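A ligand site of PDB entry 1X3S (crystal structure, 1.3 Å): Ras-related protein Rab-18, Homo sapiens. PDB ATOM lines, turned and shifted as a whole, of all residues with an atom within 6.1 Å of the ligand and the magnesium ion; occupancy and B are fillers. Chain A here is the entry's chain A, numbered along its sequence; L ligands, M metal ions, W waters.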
ATOM      1  N   GLY A  22       2.414 -26.530 -14.420  1.00  0.00           N
ATOM      2  CA  GLY A  22       1.148 -26.326 -13.724  1.00  0.00           C
ATOM      3  C   GLY A  22       0.134 -27.338 -14.206  1.00  0.00           C
ATOM      4  O   GLY A  22       0.339 -28.026 -15.209  1.00  0.00           O
ATOM      5  N   GLU A  23      -0.982 -27.407 -13.517  1.00  0.00           N
ATOM      6  CA  GLU A  23      -1.989 -28.422 -13.829  1.00  0.00           C
ATOM      7  C   GLU A  23      -2.587 -28.269 -15.203  1.00  0.00           C
ATOM      8  O   GLU A  23      -2.550 -27.201 -15.845  1.00  0.00           O
ATOM      9  CB  GLU A  23      -3.130 -28.313 -12.809  1.00  0.00           C
ATOM     10  CG  GLU A  23      -2.753 -28.747 -11.401  1.00  0.00           C
ATOM     11  CD  GLU A  23      -2.315 -30.195 -11.316  1.00  0.00           C
ATOM     12  OE1 GLU A  23      -1.140 -30.463 -11.134  1.00  0.00           O
ATOM     13  OE2 GLU A  23      -3.202 -31.032 -11.463  1.00  0.00           O
ATOM     14  N   SER A  24      -3.116 -29.390 -15.716  1.00  0.00           N
ATOM     15  CA  SER A  24      -3.742 -29.360 -16.997  1.00  0.00           C
ATOM     16  C   SER A  24      -4.906 -28.371 -16.990  1.00  0.00           C
ATOM     17  O   SER A  24      -5.670 -28.252 -15.995  1.00  0.00           O
ATOM     18  CB  SER A  24      -4.258 -30.758 -17.344  1.00  0.00           C
ATOM     19  OG  SER A  24      -4.785 -30.778 -18.644  1.00  0.00           O
ATOM     20  N   GLY A  25      -5.059 -27.650 -18.100  1.00  0.00           N
ATOM     21  CA  GLY A  25      -6.187 -26.760 -18.322  1.00  0.00           C
ATOM     22  C   GLY A  25      -6.048 -25.378 -17.721  1.00  0.00           C
ATOM     23  O   GLY A  25      -6.942 -24.553 -17.894  1.00  0.00           O
ATOM     24  N   VAL A  26      -4.916 -25.069 -17.086  1.00  0.00           N
ATOM     25  CA  VAL A  26      -4.794 -23.748 -16.453  1.00  0.00           C
ATOM     26  C   VAL A  26      -4.503 -22.628 -17.463  1.00  0.00           C
ATOM     27  O   VAL A  26      -4.663 -21.456 -17.124  1.00  0.00           O
ATOM     28  CB  VAL A  26      -3.759 -23.703 -15.332  1.00  0.00           C
ATOM     29  CG1 VAL A  26      -4.144 -24.738 -14.239  1.00  0.00           C
ATOM     30  CG2 VAL A  26      -2.348 -23.982 -15.869  1.00  0.00           C
ATOM     31  N   GLY A  27      -4.035 -23.003 -18.662  1.00  0.00           N
ATOM     32  CA  GLY A  27      -3.755 -22.021 -19.704  1.00  0.00           C
ATOM     33  C   GLY A  27      -2.272 -21.856 -20.014  1.00  0.00           C
ATOM     34  O   GLY A  27      -1.906 -20.825 -20.599  1.00  0.00           O
ATOM     35  N   LYS A  28      -1.439 -22.827 -19.696  1.00  0.00           N
ATOM     36  CA  LYS A  28      -0.007 -22.713 -20.015  1.00  0.00           C
ATOM     37  C   LYS A  28       0.239 -22.446 -21.506  1.00  0.00           C
ATOM     38  O   LYS A  28       0.937 -21.512 -21.898  1.00  0.00           O
ATOM     39  CB  LYS A  28       0.736 -23.974 -19.571  1.00  0.00           C
ATOM     40  CG  LYS A  28       0.648 -24.199 -18.077  1.00  0.00           C
ATOM     41  CD  LYS A  28       1.437 -25.408 -17.616  1.00  0.00           C
ATOM     42  CE  LYS A  28       0.999 -26.726 -18.228  1.00  0.00           C
ATOM     43  NZ  LYS A  28      -0.427 -27.040 -17.857  1.00  0.00           N
ATOM     44  N   SER A  29      -0.329 -23.316 -22.343  1.00  0.00           N
ATOM     45  CA  SER A  29      -0.141 -23.204 -23.773  1.00  0.00           C
ATOM     46  C   SER A  29      -0.789 -21.978 -24.343  1.00  0.00           C
ATOM     47  O   SER A  29      -0.272 -21.396 -25.272  1.00  0.00           O
ATOM     48  CB  SER A  29      -0.640 -24.423 -24.507  1.00  0.00           C
ATOM     49  OG  SER A  29       0.033 -25.558 -23.966  1.00  0.00           O
ATOM     50  N   SER A  30      -1.873 -21.532 -23.746  1.00  0.00           N
ATOM     51  CA  SER A  30      -2.536 -20.309 -24.212  1.00  0.00           C
ATOM     52  C   SER A  30      -1.700 -19.095 -23.851  1.00  0.00           C
ATOM     53  O   SER A  30      -1.587 -18.136 -24.652  1.00  0.00           O
ATOM     54  CB  SER A  30      -3.939 -20.194 -23.626  1.00  0.00           C
ATOM     55  OG  SER A  30      -4.778 -21.248 -24.134  1.00  0.00           O
ATOM     56  N   LEU A  31      -1.120 -19.060 -22.651  1.00  0.00           N
ATOM     57  CA  LEU A  31      -0.249 -17.936 -22.330  1.00  0.00           C
ATOM     58  C   LEU A  31       0.915 -17.908 -23.333  1.00  0.00           C
ATOM     59  O   LEU A  31       1.271 -16.817 -23.830  1.00  0.00           O
ATOM     60  CB  LEU A  31       0.286 -18.062 -20.893  1.00  0.00           C
ATOM     61  CG  LEU A  31      -0.767 -17.835 -19.804  1.00  0.00           C
ATOM     62  CD1 LEU A  31      -0.271 -18.416 -18.478  1.00  0.00           C
ATOM     63  CD2 LEU A  31      -1.055 -16.328 -19.676  1.00  0.00           C
ATOM     64  N   PHE A  40      -5.388 -16.217 -29.549  1.00  0.00           N
ATOM     65  CA  PHE A  40      -6.031 -17.066 -28.575  1.00  0.00           C
ATOM     66  C   PHE A  40      -6.883 -18.114 -29.297  1.00  0.00           C
ATOM     67  O   PHE A  40      -7.540 -17.801 -30.301  1.00  0.00           O
ATOM     68  CB  PHE A  40      -6.912 -16.203 -27.673  1.00  0.00           C
ATOM     69  CG  PHE A  40      -7.717 -16.976 -26.655  1.00  0.00           C
ATOM     70  CD1 PHE A  40      -7.106 -17.509 -25.525  1.00  0.00           C
ATOM     71  CD2 PHE A  40      -9.094 -17.200 -26.816  1.00  0.00           C
ATOM     72  CE1 PHE A  40      -7.794 -18.222 -24.600  1.00  0.00           C
ATOM     73  CE2 PHE A  40      -9.816 -17.916 -25.892  1.00  0.00           C
ATOM     74  CZ  PHE A  40      -9.170 -18.445 -24.760  1.00  0.00           C
ATOM     75  N   ASP A  41      -6.865 -19.347 -28.824  1.00  0.00           N
ATOM     76  CA  ASP A  41      -7.609 -20.451 -29.418  1.00  0.00           C
ATOM     77  C   ASP A  41      -8.483 -21.016 -28.297  1.00  0.00           C
ATOM     78  O   ASP A  41      -8.012 -21.686 -27.376  1.00  0.00           O
ATOM     79  CB  ASP A  41      -6.660 -21.510 -29.955  1.00  0.00           C
ATOM     80  CG  ASP A  41      -7.380 -22.644 -30.641  1.00  0.00           C
ATOM     81  OD1 ASP A  41      -8.628 -22.692 -30.541  1.00  0.00           O
ATOM     82  OD2 ASP A  41      -6.685 -23.474 -31.259  1.00  0.00           O
ATOM     83  N   PRO A  42      -9.798 -20.765 -28.370  1.00  0.00           N
ATOM     84  CA  PRO A  42     -10.725 -21.255 -27.350  1.00  0.00           C
ATOM     85  C   PRO A  42     -10.791 -22.768 -27.257  1.00  0.00           C
ATOM     86  O   PRO A  42     -11.232 -23.330 -26.270  1.00  0.00           O
ATOM     87  CB  PRO A  42     -12.089 -20.675 -27.787  1.00  0.00           C
ATOM     88  CG  PRO A  42     -11.747 -19.526 -28.683  1.00  0.00           C
ATOM     89  CD  PRO A  42     -10.463 -19.918 -29.384  1.00  0.00           C
ATOM     90  N   GLU A  43     -10.343 -23.426 -28.329  1.00  0.00           N
ATOM     91  CA  GLU A  43     -10.350 -24.860 -28.426  1.00  0.00           C
ATOM     92  C   GLU A  43      -8.953 -25.461 -28.483  1.00  0.00           C
ATOM     93  O   GLU A  43      -8.786 -26.561 -28.977  1.00  0.00           O
ATOM     94  CB  GLU A  43     -11.154 -25.334 -29.654  1.00  0.00           C
ATOM     95  CG  GLU A  43     -12.515 -24.647 -29.808  1.00  0.00           C
ATOM     96  CD  GLU A  43     -13.441 -24.944 -28.654  1.00  0.00           C
ATOM     97  OE1 GLU A  43     -14.305 -24.085 -28.374  1.00  0.00           O
ATOM     98  OE2 GLU A  43     -13.314 -26.017 -28.023  1.00  0.00           O
ATOM     99  N   LEU A  44      -7.969 -24.738 -27.942  1.00  0.00           N
ATOM    100  CA  LEU A  44      -6.584 -25.246 -27.967  1.00  0.00           C
ATOM    101  C   LEU A  44      -6.495 -26.661 -27.394  1.00  0.00           C
ATOM    102  O   LEU A  44      -7.030 -26.939 -26.345  1.00  0.00           O
ATOM    103  CB  LEU A  44      -5.687 -24.300 -27.161  1.00  0.00           C
ATOM    104  CG  LEU A  44      -4.198 -24.529 -27.375  1.00  0.00           C
ATOM    105  CD1 LEU A  44      -3.846 -24.273 -28.871  1.00  0.00           C
ATOM    106  CD2 LEU A  44      -3.405 -23.550 -26.527  1.00  0.00           C
ATOM    107  N   ALA A  45      -5.812 -27.556 -28.117  1.00  0.00           N
ATOM    108  CA  ALA A  45      -5.643 -28.927 -27.665  1.00  0.00           C
ATOM    109  C   ALA A  45      -4.705 -29.104 -26.469  1.00  0.00           C
ATOM    110  O   ALA A  45      -3.723 -28.365 -26.326  1.00  0.00           O
ATOM    111  CB  ALA A  45      -5.151 -29.780 -28.834  1.00  0.00           C
ATOM    112  N   ALA A  46      -5.004 -30.033 -25.587  1.00  0.00           N
ATOM    113  CA  ALA A  46      -4.149 -30.365 -24.466  1.00  0.00           C
ATOM    114  C   ALA A  46      -2.806 -30.752 -25.031  1.00  0.00           C
ATOM    115  O   ALA A  46      -2.706 -31.425 -26.080  1.00  0.00           O
ATOM    116  CB  ALA A  46      -4.719 -31.536 -23.656  1.00  0.00           C
ATOM    117  N   THR A  47      -1.754 -30.378 -24.313  1.00  0.00           N
ATOM    118  CA  THR A  47      -0.393 -30.669 -24.696  1.00  0.00           C
ATOM    119  C   THR A  47      -0.050 -32.100 -24.357  1.00  0.00           C
ATOM    120  O   THR A  47      -0.314 -32.566 -23.242  1.00  0.00           O
ATOM    121  CB  THR A  47       0.534 -29.714 -23.932  1.00  0.00           C
ATOM    122  OG1 THR A  47       0.119 -28.359 -24.244  1.00  0.00           O
ATOM    123  CG2 THR A  47       1.973 -29.871 -24.346  1.00  0.00           C
ATOM    124  N   ILE A  48       0.594 -32.772 -25.324  1.00  0.00           N
ATOM    125  CA  ILE A  48       1.089 -34.138 -25.114  1.00  0.00           C
ATOM    126  C   ILE A  48       2.626 -33.995 -25.126  1.00  0.00           C
ATOM    127  O   ILE A  48       3.204 -33.475 -26.078  1.00  0.00           O
ATOM    128  CB  ILE A  48       0.613 -35.078 -26.254  1.00  0.00           C
ATOM    129  CG1 ILE A  48      -0.930 -35.107 -26.285  1.00  0.00           C
ATOM    130  CG2 ILE A  48       1.237 -36.448 -26.070  1.00  0.00           C
ATOM    131  CD1 ILE A  48      -1.590 -35.863 -27.485  1.00  0.00           C
ATOM    132  N   ASP A  70       7.031 -25.832 -22.853  1.00  0.00           N
ATOM    133  CA  ASP A  70       5.664 -25.842 -22.379  1.00  0.00           C
ATOM    134  C   ASP A  70       5.308 -27.302 -22.136  1.00  0.00           C
ATOM    135  O   ASP A  70       5.188 -28.058 -23.068  1.00  0.00           O
ATOM    136  CB  ASP A  70       4.780 -25.195 -23.429  1.00  0.00           C
ATOM    137  CG  ASP A  70       3.308 -25.313 -23.102  1.00  0.00           C
ATOM    138  OD1 ASP A  70       2.957 -25.513 -21.917  1.00  0.00           O
ATOM    139  OD2 ASP A  70       2.545 -25.184 -24.093  1.00  0.00           O
ATOM    140  N   THR A  71       5.120 -27.697 -20.893  1.00  0.00           N
ATOM    141  CA  THR A  71       4.864 -29.085 -20.604  1.00  0.00           C
ATOM    142  C   THR A  71       3.436 -29.475 -20.432  1.00  0.00           C
ATOM    143  O   THR A  71       2.562 -28.677 -20.166  1.00  0.00           O
ATOM    144  CB  THR A  71       5.675 -29.466 -19.372  1.00  0.00           C
ATOM    145  OG1 THR A  71       5.149 -28.807 -18.209  1.00  0.00           O
ATOM    146  CG2 THR A  71       7.178 -29.091 -19.625  1.00  0.00           C
ATOM    147  N   ALA A  72       3.150 -30.757 -20.585  1.00  0.00           N
ATOM    148  CA  ALA A  72       1.809 -31.253 -20.384  1.00  0.00           C
ATOM    149  C   ALA A  72       1.507 -31.209 -18.868  1.00  0.00           C
ATOM    150  O   ALA A  72       2.352 -31.543 -18.046  1.00  0.00           O
ATOM    151  CB  ALA A  72       1.677 -32.709 -20.883  1.00  0.00           C
ATOM    152  N   GLY A  73       0.295 -30.758 -18.499  1.00  0.00           N
ATOM    153  CA  GLY A  73      -0.128 -30.751 -17.099  1.00  0.00           C
ATOM    154  C   GLY A  73      -0.582 -32.126 -16.623  1.00  0.00           C
ATOM    155  O   GLY A  73      -0.576 -32.399 -15.394  1.00  0.00           O
ATOM    156  N   GLN A  74      -0.955 -33.000 -17.562  1.00  0.00           N
ATOM    157  CA  GLN A  74      -1.400 -34.376 -17.206  1.00  0.00           C
ATOM    158  C   GLN A  74      -0.139 -35.247 -17.047  1.00  0.00           C
ATOM    159  O   GLN A  74       0.618 -35.461 -18.001  1.00  0.00           O
ATOM    160  CB  GLN A  74      -2.291 -34.928 -18.303  1.00  0.00           C
ATOM    161  CG  GLN A  74      -3.600 -34.195 -18.471  1.00  0.00           C
ATOM    162  CD  GLN A  74      -4.388 -34.716 -19.656  1.00  0.00           C
ATOM    163  OE1 GLN A  74      -5.263 -35.575 -19.512  1.00  0.00           O
ATOM    164  NE2 GLN A  74      -4.075 -34.208 -20.839  1.00  0.00           N
ATOM    165  N   ASN A 129      -3.897 -17.338 -13.936  1.00  0.00           N
ATOM    166  CA  ASN A 129      -4.500 -17.112 -15.233  1.00  0.00           C
ATOM    167  C   ASN A 129      -6.039 -17.196 -15.216  1.00  0.00           C
ATOM    168  O   ASN A 129      -6.654 -17.652 -14.249  1.00  0.00           O
ATOM    169  CB  ASN A 129      -3.896 -18.117 -16.209  1.00  0.00           C
ATOM    170  CG  ASN A 129      -4.248 -17.872 -17.668  1.00  0.00           C
ATOM    171  OD1 ASN A 129      -4.579 -18.842 -18.424  1.00  0.00           O
ATOM    172  ND2 ASN A 129      -4.195 -16.653 -18.072  1.00  0.00           N
ATOM    173  N   LYS A 130      -6.621 -16.717 -16.306  1.00  0.00           N
ATOM    174  CA  LYS A 130      -8.066 -16.750 -16.526  1.00  0.00           C
ATOM    175  C   LYS A 130      -8.804 -15.712 -15.708  1.00  0.00           C
ATOM    176  O   LYS A 130      -9.962 -15.937 -15.341  1.00  0.00           O
ATOM    177  CB  LYS A 130      -8.671 -18.152 -16.357  1.00  0.00           C
ATOM    178  CG  LYS A 130      -7.929 -19.236 -17.116  1.00  0.00           C
ATOM    179  CD  LYS A 130      -8.877 -20.394 -17.455  1.00  0.00           C
ATOM    180  CE  LYS A 130      -8.125 -21.607 -17.952  1.00  0.00           C
ATOM    181  NZ  LYS A 130      -9.095 -22.707 -18.391  1.00  0.00           N
ATOM    182  N   ILE A 131      -8.165 -14.578 -15.455  1.00  0.00           N
ATOM    183  CA  ILE A 131      -8.848 -13.566 -14.654  1.00  0.00           C
ATOM    184  C   ILE A 131     -10.039 -12.950 -15.381  1.00  0.00           C
ATOM    185  O   ILE A 131     -10.843 -12.232 -14.747  1.00  0.00           O
ATOM    186  CB  ILE A 131      -7.885 -12.470 -14.156  1.00  0.00           C
ATOM    187  CG1 ILE A 131      -7.270 -11.683 -15.323  1.00  0.00           C
ATOM    188  CG2 ILE A 131      -6.768 -13.121 -13.306  1.00  0.00           C
ATOM    189  CD1 ILE A 131      -6.388 -10.521 -14.922  1.00  0.00           C
ATOM    190  N   ASP A 132     -10.195 -13.198 -16.660  1.00  0.00           N
ATOM    191  CA  ASP A 132     -11.380 -12.718 -17.419  1.00  0.00           C
ATOM    192  C   ASP A 132     -12.645 -13.519 -17.114  1.00  0.00           C
ATOM    193  O   ASP A 132     -13.768 -13.036 -17.379  1.00  0.00           O
ATOM    194  CB  ASP A 132     -11.108 -12.893 -18.920  1.00  0.00           C
ATOM    195  CG  ASP A 132     -10.892 -14.321 -19.303  1.00  0.00           C
ATOM    196  OD1 ASP A 132      -9.764 -14.850 -19.016  1.00  0.00           O
ATOM    197  OD2 ASP A 132     -11.761 -14.988 -19.848  1.00  0.00           O
ATOM    198  N   LYS A 133     -12.508 -14.701 -16.566  1.00  0.00           N
ATOM    199  CA  LYS A 133     -13.636 -15.606 -16.360  1.00  0.00           C
ATOM    200  C   LYS A 133     -14.460 -15.375 -15.130  1.00  0.00           C
ATOM    201  O   LYS A 133     -13.996 -14.826 -14.126  1.00  0.00           O
ATOM    202  CB  LYS A 133     -13.135 -17.035 -16.291  1.00  0.00           C
ATOM    203  CG  LYS A 133     -12.685 -17.611 -17.611  1.00  0.00           C
ATOM    204  CD  LYS A 133     -12.389 -19.129 -17.503  1.00  0.00           C
ATOM    205  CE  LYS A 133     -13.607 -20.006 -17.764  1.00  0.00           C
ATOM    206  NZ  LYS A 133     -13.263 -21.462 -17.778  1.00  0.00           N
ATOM    207  N   ALA A 157      -3.041 -12.887 -14.914  1.00  0.00           N
ATOM    208  CA  ALA A 157      -3.127 -12.724 -16.360  1.00  0.00           C
ATOM    209  C   ALA A 157      -4.394 -13.312 -16.932  1.00  0.00           C
ATOM    210  O   ALA A 157      -5.133 -14.071 -16.284  1.00  0.00           O
ATOM    211  CB  ALA A 157      -1.862 -13.479 -17.051  1.00  0.00           C
ATOM    212  N   SER A 158      -4.634 -12.934 -18.189  1.00  0.00           N
ATOM    213  CA  SER A 158      -5.626 -13.583 -19.011  1.00  0.00           C
ATOM    214  C   SER A 158      -5.027 -13.790 -20.393  1.00  0.00           C
ATOM    215  O   SER A 158      -4.748 -12.792 -21.093  1.00  0.00           O
ATOM    216  CB  SER A 158      -6.909 -12.767 -19.181  1.00  0.00           C
ATOM    217  OG  SER A 158      -7.753 -13.408 -20.129  1.00  0.00           O
ATOM    218  N   ALA A 159      -4.839 -15.043 -20.790  1.00  0.00           N
ATOM    219  CA  ALA A 159      -4.359 -15.284 -22.160  1.00  0.00           C
ATOM    220  C   ALA A 159      -5.456 -14.801 -23.143  1.00  0.00           C
ATOM    221  O   ALA A 159      -5.155 -14.400 -24.274  1.00  0.00           O
ATOM    222  CB  ALA A 159      -4.094 -16.764 -22.360  1.00  0.00           C
ATOM    223  N   LYS A 160      -6.718 -14.858 -22.710  1.00  0.00           N
ATOM    224  CA  LYS A 160      -7.829 -14.528 -23.611  1.00  0.00           C
ATOM    225  C   LYS A 160      -7.913 -13.034 -23.895  1.00  0.00           C
ATOM    226  O   LYS A 160      -8.090 -12.656 -25.078  1.00  0.00           O
ATOM    227  CB  LYS A 160      -9.124 -15.055 -23.002  1.00  0.00           C
ATOM    228  CG  LYS A 160     -10.340 -14.850 -23.959  1.00  0.00           C
ATOM    229  CD  LYS A 160     -11.556 -15.546 -23.373  1.00  0.00           C
ATOM    230  CE  LYS A 160     -12.866 -15.329 -24.138  1.00  0.00           C
ATOM    231  NZ  LYS A 160     -13.989 -16.011 -23.390  1.00  0.00           N
ATOM    232  N   THR A 161      -7.734 -12.206 -22.887  1.00  0.00           N
ATOM    233  CA  THR A 161      -7.817 -10.744 -23.040  1.00  0.00           C
ATOM    234  C   THR A 161      -6.520 -10.013 -22.905  1.00  0.00           C
ATOM    235  O   THR A 161      -6.505  -8.797 -22.778  1.00  0.00           O
ATOM    236  CB  THR A 161      -8.819 -10.108 -22.042  1.00  0.00           C
ATOM    237  OG1 THR A 161      -8.346 -10.271 -20.714  1.00  0.00           O
ATOM    238  CG2 THR A 161     -10.186 -10.739 -22.179  1.00  0.00           C
HETATM  239  P1  LIG L   1      -2.398 -28.879 -20.682  1.00  0.00           P
HETATM  240  O1  LIG L   1      -3.364 -30.054 -20.728  1.00  0.00           O
HETATM  241  O2  LIG L   1      -1.650 -28.755 -22.020  1.00  0.00           O
HETATM  242  O3  LIG L   1      -1.507 -28.963 -19.468  1.00  0.00           O
HETATM  243  N1  LIG L   1      -3.432 -27.535 -20.457  1.00  0.00           N
HETATM  244  P2  LIG L   1      -2.833 -25.952 -20.587  1.00  0.00           P
HETATM  245  O4  LIG L   1      -2.443 -25.498 -19.209  1.00  0.00           O
HETATM  246  O5  LIG L   1      -1.771 -25.778 -21.673  1.00  0.00           O
HETATM  247  O6  LIG L   1      -4.196 -25.191 -20.991  1.00  0.00           O
HETATM  248  P3  LIG L   1      -4.588 -24.489 -22.389  1.00  0.00           P
HETATM  249  O7  LIG L   1      -3.757 -23.366 -22.748  1.00  0.00           O
HETATM  250  O8  LIG L   1      -4.693 -25.639 -23.382  1.00  0.00           O
HETATM  251  O9  LIG L   1      -6.043 -23.909 -22.032  1.00  0.00           O
HETATM  252  C1  LIG L   1      -7.117 -24.863 -21.626  1.00  0.00           C
HETATM  253  C2  LIG L   1      -8.504 -24.204 -22.013  1.00  0.00           C
HETATM  254  O10 LIG L   1      -8.591 -22.949 -21.295  1.00  0.00           O
HETATM  255  C3  LIG L   1      -8.450 -23.897 -23.442  1.00  0.00           C
HETATM  256  O11 LIG L   1      -9.768 -24.163 -24.074  1.00  0.00           O
HETATM  257  C4  LIG L   1      -8.211 -22.403 -23.626  1.00  0.00           C
HETATM  258  O12 LIG L   1      -8.944 -21.719 -24.613  1.00  0.00           O
HETATM  259  C5  LIG L   1      -8.677 -21.907 -22.221  1.00  0.00           C
HETATM  260  N2  LIG L   1      -8.014 -20.747 -21.697  1.00  0.00           N
HETATM  261  C6  LIG L   1      -6.628 -20.592 -21.560  1.00  0.00           C
HETATM  262  N3  LIG L   1      -6.354 -19.441 -21.033  1.00  0.00           N
HETATM  263  C7  LIG L   1      -7.539 -18.803 -20.803  1.00  0.00           C
HETATM  264  C8  LIG L   1      -7.860 -17.551 -20.254  1.00  0.00           C
HETATM  265  O13 LIG L   1      -7.030 -16.720 -19.883  1.00  0.00           O
HETATM  266  N4  LIG L   1      -9.176 -17.238 -20.155  1.00  0.00           N
HETATM  267  C9  LIG L   1     -10.169 -18.105 -20.573  1.00  0.00           C
HETATM  268  N5  LIG L   1     -11.464 -17.690 -20.418  1.00  0.00           N
HETATM  269  N6  LIG L   1      -9.909 -19.294 -21.099  1.00  0.00           N
HETATM  270  C10 LIG L   1      -8.598 -19.656 -21.222  1.00  0.00           C
HETATM  271 MG    MG M   1      -0.854 -27.137 -22.903  1.00  0.00          MG
HETATM  272  O   HOH W   1      -1.757 -32.304 -20.780  1.00  0.00           O
HETATM  273  O   HOH W   2      -6.370 -27.666 -23.755  1.00  0.00           O
HETATM  274  O   HOH W   3      -5.968 -28.934 -21.439  1.00  0.00           O
HETATM  275  O   HOH W   4       0.859 -27.101 -21.646  1.00  0.00           O
HETATM  276  O   HOH W   5      -9.565 -26.840 -25.381  1.00  0.00           O
HETATM  277  O   HOH W   6      -2.522 -27.007 -24.231  1.00  0.00           O
HETATM  278  O   HOH W   7     -11.274 -21.539 -19.959  1.00  0.00           O
HETATM  279  O   HOH W   8     -13.743 -18.966 -21.555  1.00  0.00           O
HETATM  280  O   HOH W   9      -9.926 -25.554 -19.203  1.00  0.00           O
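The side-chain amino group (NZ) of Lys 28 lies within hydrogen-bond range of the backbone carbonyl oxygen (O) of Gly 22, 2.9 Å away.
ND2 of Asn 129 sits close to N of Ala 159, 3.2 Å away.
OD1 of Asp 41 sits at hydrogen-bond distance from N of Leu 44, at 3.4 Å.
The backbone NH (N) of Glu 43 sits at hydrogen-bond distance from the side-chain carboxylate (OD1) of Asp 41 (2.9 Å).
The backbone carbonyl oxygen of Ala 157 lies within hydrogen-bond range of the backbone NH of Lys 130 (3.0 Å).
ND2 of Asn 129 sits at hydrogen-bond distance from O of Ala 157 (3.3 Å).
The backbone NH (N) of Lys 160 sits close to the side-chain hydroxyl (OG) of Ser 158, at 3.1 Å.
The side-chain hydroxyl (OG) of Ser 158 sits at hydrogen-bond distance from the backbone NH (N) of Thr 161 (3.0 Å).
N of Gly 25 sits close to N1 of the ligand.
Residues that only touch the ligand: Glu 23 (3.8 Å), Phe 40 (3.3 Å), Leu 44 (3.8 Å), Ala 46 (3.6 Å), Ala 72 (3.8 Å) and Lys 133 (3.1 Å).
Hydrophobic or aromatic side chains within 4 Å of the ligand: Val 26, Phe 40, Leu 44, Ala 46 and Ala 159.
Within 4 Å of the ligand: Glu 23, Ser 24, Gly 25, Val 26, Gly 27, Lys 28, Ser 29, Ser 30, Phe 40, Asp 41, Pro 42, Leu 44, Ala 46, Thr 47, Ala 72, Gly 73, Asn 129, Lys 130, Asp 132, Lys 133, Ser 158, Ala 159 and Lys 160.
O2 of the ligand lies close to N of Thr 47, at 2.8 Å.
N of Ser 29 lies within hydrogen-bond range of O7 of the ligand (3.5 Å).
The side-chain hydroxyl of Ser 24 sits at hydrogen-bond distance from an oxygen (O1) of the ligand, 2.6 Å away.
OD1 of Asp 132 sits at hydrogen-bond distance from N4 of the ligand (2.7 Å).
The backbone NH (N) of Gly 73 is in hydrogen-bond range of an oxygen (O3) of the ligand, 2.7 Å away.
O7 of the ligand sits at hydrogen-bond distance from N of Ser 30, at 2.8 Å.
The side-chain hydroxyl (OG) of Ser 30 lies within hydrogen-bond range of an oxygen (O7) of the ligand.
The backbone NH (N) of Lys 28 sits at hydrogen-bond distance from an oxygen (O4) of the ligand, at 2.9 Å.
O3 of the ligand lies within salt-bridge range of NZ of Lys 28.
O11 of the ligand sits at hydrogen-bond distance from O of Pro 42, 2.8 Å away.
An oxygen (O13) of the ligand lies within hydrogen-bond range of the backbone NH (N) of Ala 159, at 2.9 Å.
O of Asp 41 sits at hydrogen-bond distance from O12 of the ligand.
O10 of the ligand sits at hydrogen-bond distance from NZ of Lys 130.
An oxygen (O4) of the ligand sits at hydrogen-bond distance from the backbone NH of Gly 27 (3.0 Å).
OD1 of Asn 129 sits close to N3 of the ligand (3.2 Å).
The backbone NH (N) of Val 26 sits at hydrogen-bond distance from an oxygen (O4) of the ligand (3.3 Å).
O13 of the ligand is in hydrogen-bond range of OG of Ser 158 (3.4 Å).
An oxygen (O13) of the ligand is in hydrogen-bond range of the backbone NH of Lys 160 (3.4 Å).
The magnesium ion is bound by an oxygen (O2) of the ligand (2.0 Å), an oxygen (O5) of the ligand (2.0 Å), the side-chain hydroxyl (OG1) of Thr 47 (2.1 Å), the side-chain hydroxyl (OG) of Ser 29 (2.1 Å), water W4 (2.1 Å) and water W6 (2.1 Å).
Within 4 Å of the magnesium ion: Ser 29 and Thr 47.
Water W4 lies within hydrogen-bond range of OD1 of Asp 70 (2.6 Å) and O of Thr 71 (2.8 Å).
Water W2 lies within hydrogen-bond range of an oxygen (O8) of the ligand (2.7 Å), the backbone carbonyl oxygen (O) of Leu 44 (2.8 Å) and the backbone NH (N) of Ala 46 (3.3 Å).
Water W1 lies within hydrogen-bond range of an oxygen (O1) of the ligand, the backbone carbonyl oxygen (O) of Thr 47, the side-chain amide nitrogen (NE2) of Gln 74 and the backbone NH (N) of Gly 73.
Water W8 lies within hydrogen-bond range of a nitrogen (N5) of the ligand (2.8 Å) and the side-chain amino group (NZ) of Lys 160 (3.5 Å).
Water W5 bridges O of Leu 44 (2.7 Å) and O11 of the ligand (3.0 Å).
Water W9 lies within hydrogen-bond range of the side-chain amino group (NZ) of Lys 130 (3.1 Å) and the backbone carbonyl oxygen (O) of Gly 25 (3.4 Å).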
